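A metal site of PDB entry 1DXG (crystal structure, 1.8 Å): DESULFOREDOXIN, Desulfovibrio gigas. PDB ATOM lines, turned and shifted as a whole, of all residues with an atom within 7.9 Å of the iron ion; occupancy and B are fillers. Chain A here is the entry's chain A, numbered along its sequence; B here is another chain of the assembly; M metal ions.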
ATOM      1  N   LYS A   8     -23.362  24.084   0.457  1.00  0.00           N
ATOM      2  CA  LYS A   8     -22.111  24.638  -0.052  1.00  0.00           C
ATOM      3  C   LYS A   8     -21.901  24.261  -1.499  1.00  0.00           C
ATOM      4  O   LYS A   8     -22.201  23.133  -1.877  1.00  0.00           O
ATOM      5  CB  LYS A   8     -20.943  24.094   0.733  1.00  0.00           C
ATOM      6  CG  LYS A   8     -19.571  24.659   0.343  1.00  0.00           C
ATOM      7  CD  LYS A   8     -18.542  23.824   1.069  1.00  0.00           C
ATOM      8  CE  LYS A   8     -17.170  24.411   0.841  1.00  0.00           C
ATOM      9  NZ  LYS A   8     -16.162  23.471   1.340  1.00  0.00           N
ATOM     10  N   CYS A   9     -21.429  25.163  -2.345  1.00  0.00           N
ATOM     11  CA  CYS A   9     -21.005  24.822  -3.697  1.00  0.00           C
ATOM     12  C   CYS A   9     -19.533  24.406  -3.604  1.00  0.00           C
ATOM     13  O   CYS A   9     -18.674  25.236  -3.264  1.00  0.00           O
ATOM     14  CB  CYS A   9     -21.107  26.000  -4.659  1.00  0.00           C
ATOM     15  SG  CYS A   9     -20.374  25.638  -6.274  1.00  0.00           S
ATOM     16  N   GLU A  10     -19.175  23.182  -3.946  1.00  0.00           N
ATOM     17  CA  GLU A  10     -17.794  22.733  -3.850  1.00  0.00           C
ATOM     18  C   GLU A  10     -16.843  23.417  -4.826  1.00  0.00           C
ATOM     19  O   GLU A  10     -15.639  23.483  -4.585  1.00  0.00           O
ATOM     20  CB  GLU A  10     -17.723  21.225  -4.069  1.00  0.00           C
ATOM     21  CG  GLU A  10     -18.482  20.363  -3.045  1.00  0.00           C
ATOM     22  CD  GLU A  10     -18.044  20.435  -1.576  1.00  0.00           C
ATOM     23  OE1 GLU A  10     -16.985  20.963  -1.251  1.00  0.00           O
ATOM     24  OE2 GLU A  10     -18.779  19.942  -0.724  1.00  0.00           O
ATOM     25  N   LEU A  11     -17.334  23.922  -5.953  1.00  0.00           N
ATOM     26  CA  LEU A  11     -16.465  24.530  -6.937  1.00  0.00           C
ATOM     27  C   LEU A  11     -16.129  25.992  -6.687  1.00  0.00           C
ATOM     28  O   LEU A  11     -14.951  26.329  -6.721  1.00  0.00           O
ATOM     29  CB  LEU A  11     -17.126  24.355  -8.301  1.00  0.00           C
ATOM     30  CG  LEU A  11     -17.393  22.894  -8.617  1.00  0.00           C
ATOM     31  CD1 LEU A  11     -18.122  22.773  -9.933  1.00  0.00           C
ATOM     32  CD2 LEU A  11     -16.079  22.132  -8.641  1.00  0.00           C
ATOM     33  N   CYS A  12     -17.082  26.836  -6.322  1.00  0.00           N
ATOM     34  CA  CYS A  12     -16.778  28.255  -6.117  1.00  0.00           C
ATOM     35  C   CYS A  12     -16.808  28.651  -4.635  1.00  0.00           C
ATOM     36  O   CYS A  12     -16.506  29.810  -4.343  1.00  0.00           O
ATOM     37  CB  CYS A  12     -17.772  29.154  -6.905  1.00  0.00           C
ATOM     38  SG  CYS A  12     -19.473  29.237  -6.269  1.00  0.00           S
ATOM     39  N   GLY A  13     -17.172  27.755  -3.703  1.00  0.00           N
ATOM     40  CA  GLY A  13     -17.155  28.015  -2.262  1.00  0.00           C
ATOM     41  C   GLY A  13     -18.353  28.791  -1.722  1.00  0.00           C
ATOM     42  O   GLY A  13     -18.370  29.135  -0.544  1.00  0.00           O
ATOM     43  N   GLN A  14     -19.382  29.062  -2.522  1.00  0.00           N
ATOM     44  CA  GLN A  14     -20.523  29.844  -2.058  1.00  0.00           C
ATOM     45  C   GLN A  14     -21.315  28.988  -1.068  1.00  0.00           C
ATOM     46  O   GLN A  14     -21.526  27.789  -1.310  1.00  0.00           O
ATOM     47  CB  GLN A  14     -21.382  30.244  -3.274  1.00  0.00           C
ATOM     48  CG  GLN A  14     -22.593  31.105  -2.984  1.00  0.00           C
ATOM     49  CD  GLN A  14     -23.036  31.892  -4.189  1.00  0.00           C
ATOM     50  OE1 GLN A  14     -23.257  33.091  -4.119  1.00  0.00           O
ATOM     51  NE2 GLN A  14     -23.168  31.316  -5.371  1.00  0.00           N
ATOM     52  N   VAL A  15     -21.746  29.597   0.041  1.00  0.00           N
ATOM     53  CA  VAL A  15     -22.463  28.879   1.085  1.00  0.00           C
ATOM     54  C   VAL A  15     -23.801  29.567   1.285  1.00  0.00           C
ATOM     55  O   VAL A  15     -23.788  30.791   1.449  1.00  0.00           O
ATOM     56  CB  VAL A  15     -21.689  28.888   2.439  1.00  0.00           C
ATOM     57  CG1 VAL A  15     -22.422  28.059   3.463  1.00  0.00           C
ATOM     58  CG2 VAL A  15     -20.335  28.242   2.294  1.00  0.00           C
ATOM     59  N   VAL A  27     -28.531  24.370  -7.199  1.00  0.00           N
ATOM     60  CA  VAL A  27     -27.414  24.131  -8.095  1.00  0.00           C
ATOM     61  C   VAL A  27     -26.572  25.379  -8.168  1.00  0.00           C
ATOM     62  O   VAL A  27     -27.094  26.503  -8.140  1.00  0.00           O
ATOM     63  CB  VAL A  27     -27.927  23.773  -9.512  1.00  0.00           C
ATOM     64  CG1 VAL A  27     -26.822  23.720 -10.569  1.00  0.00           C
ATOM     65  CG2 VAL A  27     -28.601  22.423  -9.417  1.00  0.00           C
ATOM     66  N   CYS A  28     -25.256  25.209  -8.277  1.00  0.00           N
ATOM     67  CA  CYS A  28     -24.337  26.311  -8.420  1.00  0.00           C
ATOM     68  C   CYS A  28     -23.168  25.790  -9.229  1.00  0.00           C
ATOM     69  O   CYS A  28     -22.729  24.669  -8.984  1.00  0.00           O
ATOM     70  CB  CYS A  28     -23.851  26.798  -7.056  1.00  0.00           C
ATOM     71  SG  CYS A  28     -22.841  28.296  -7.149  1.00  0.00           S
ATOM     72  N   CYS A  29     -22.652  26.534 -10.216  1.00  0.00           N
ATOM     73  CA  CYS A  29     -21.495  26.122 -11.039  1.00  0.00           C
ATOM     74  C   CYS A  29     -21.737  24.810 -11.801  1.00  0.00           C
ATOM     75  O   CYS A  29     -20.851  23.975 -12.005  1.00  0.00           O
ATOM     76  CB  CYS A  29     -20.247  25.968 -10.153  1.00  0.00           C
ATOM     77  SG  CYS A  29     -19.683  27.530  -9.457  1.00  0.00           S
ATOM     78  N   GLY A  30     -22.962  24.588 -12.272  1.00  0.00           N
ATOM     79  CA  GLY A  30     -23.334  23.387 -12.999  1.00  0.00           C
ATOM     80  C   GLY A  30     -23.392  22.152 -12.131  1.00  0.00           C
ATOM     81  O   GLY A  30     -23.425  21.044 -12.683  1.00  0.00           O
ATOM     82  N   GLU A  31     -23.417  22.221 -10.807  1.00  0.00           N
ATOM     83  CA  GLU A  31     -23.410  21.028  -9.963  1.00  0.00           C
ATOM     84  C   GLU A  31     -24.313  21.211  -8.747  1.00  0.00           C
ATOM     85  O   GLU A  31     -24.532  22.348  -8.319  1.00  0.00           O
ATOM     86  CB  GLU A  31     -21.954  20.830  -9.576  1.00  0.00           C
ATOM     87  CG  GLU A  31     -21.627  19.979  -8.380  1.00  0.00           C
ATOM     88  CD  GLU A  31     -20.128  19.905  -8.143  1.00  0.00           C
ATOM     89  OE1 GLU A  31     -19.430  19.413  -9.026  1.00  0.00           O
ATOM     90  OE2 GLU A  31     -19.675  20.327  -7.070  1.00  0.00           O
ATOM     91  N   MET A  33     -25.468  21.585  -5.065  1.00  0.00           N
ATOM     92  CA  MET A  33     -24.832  22.048  -3.847  1.00  0.00           C
ATOM     93  C   MET A  33     -24.886  20.927  -2.805  1.00  0.00           C
ATOM     94  O   MET A  33     -25.750  20.055  -2.855  1.00  0.00           O
ATOM     95  CB  MET A  33     -25.533  23.309  -3.346  1.00  0.00           C
ATOM     96  CG  MET A  33     -25.197  24.521  -4.231  1.00  0.00           C
ATOM     97  SD  MET A  33     -25.999  26.061  -3.731  1.00  0.00           S
ATOM     98  CE  MET A  33     -24.738  26.707  -2.667  1.00  0.00           C
ATOM     99  N   GLY B  22     -19.766  33.564  -3.533  1.00  0.00           N
ATOM    100  CA  GLY B  22     -19.092  32.767  -4.530  1.00  0.00           C
ATOM    101  C   GLY B  22     -19.531  33.385  -5.850  1.00  0.00           C
ATOM    102  O   GLY B  22     -20.537  34.108  -5.907  1.00  0.00           O
ATOM    103  N   GLY B  23     -18.781  33.149  -6.932  1.00  0.00           N
ATOM    104  CA  GLY B  23     -19.103  33.749  -8.213  1.00  0.00           C
ATOM    105  C   GLY B  23     -20.144  32.973  -9.016  1.00  0.00           C
ATOM    106  O   GLY B  23     -20.581  33.445 -10.074  1.00  0.00           O
ATOM    107  N   GLY B  24     -20.588  31.802  -8.549  1.00  0.00           N
ATOM    108  CA  GLY B  24     -21.533  30.975  -9.292  1.00  0.00           C
ATOM    109  C   GLY B  24     -22.938  31.551  -9.191  1.00  0.00           C
ATOM    110  O   GLY B  24     -23.221  32.233  -8.203  1.00  0.00           O
ATOM    111  N   THR B  25     -23.827  31.241 -10.148  1.00  0.00           N
ATOM    112  CA  THR B  25     -25.212  31.719 -10.132  1.00  0.00           C
ATOM    113  C   THR B  25     -26.063  30.661  -9.429  1.00  0.00           C
ATOM    114  O   THR B  25     -25.960  29.468  -9.760  1.00  0.00           O
ATOM    115  CB  THR B  25     -25.745  31.887 -11.570  1.00  0.00           C
ATOM    116  OG1 THR B  25     -24.836  32.796 -12.190  1.00  0.00           O
ATOM    117  CG2 THR B  25     -27.208  32.373 -11.654  1.00  0.00           C
ATOM    118  N   LEU B  26     -26.872  31.075  -8.454  1.00  0.00           N
ATOM    119  CA  LEU B  26     -27.728  30.149  -7.718  1.00  0.00           C
ATOM    120  C   LEU B  26     -28.896  29.736  -8.596  1.00  0.00           C
ATOM    121  O   LEU B  26     -29.604  30.588  -9.158  1.00  0.00           O
ATOM    122  CB  LEU B  26     -28.211  30.829  -6.440  1.00  0.00           C
ATOM    123  CG  LEU B  26     -27.124  31.112  -5.396  1.00  0.00           C
ATOM    124  CD1 LEU B  26     -27.738  31.904  -4.249  1.00  0.00           C
ATOM    125  CD2 LEU B  26     -26.492  29.806  -4.919  1.00  0.00           C
HETATM  126 FE    FE M   1     -20.639  27.633  -7.363  1.00  0.00          FE
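N of Gly 24 of chain B lies close to SG of Cys 12 (3.6 Å). The backbone NH of Gln 14 lies close to the side-chain sulfur of Cys 12, at 3.8 Å. The side-chain sulfur of Cys 9 lies close to the backbone NH of Leu 11 (3.5 Å). The backbone NH (N) of Cys 9 sits at hydrogen-bond distance from the backbone carbonyl oxygen (O) of Gln 14, at 2.8 Å. The side-chain sulfur (SG) of Cys 28 lies close to the side-chain amide nitrogen (NE2) of Gln 14 (3.5 Å). NE2 of Gln 14 is in hydrogen-bond range of O of Gly 24 of chain B, 3.0 Å away.
Gly 24 of chain B touches the iron ion. The nearest printed residue that does not touch the iron ion is Leu 11 (4.8 Å).
The iron ion is bound by the side-chain sulfur (SG) of Cys 12 (2.3 Å), the side-chain sulfur (SG) of Cys 9 (2.3 Å), the side-chain sulfur (SG) of Cys 29 (2.3 Å) and the side-chain sulfur (SG) of Cys 28 (2.3 Å).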
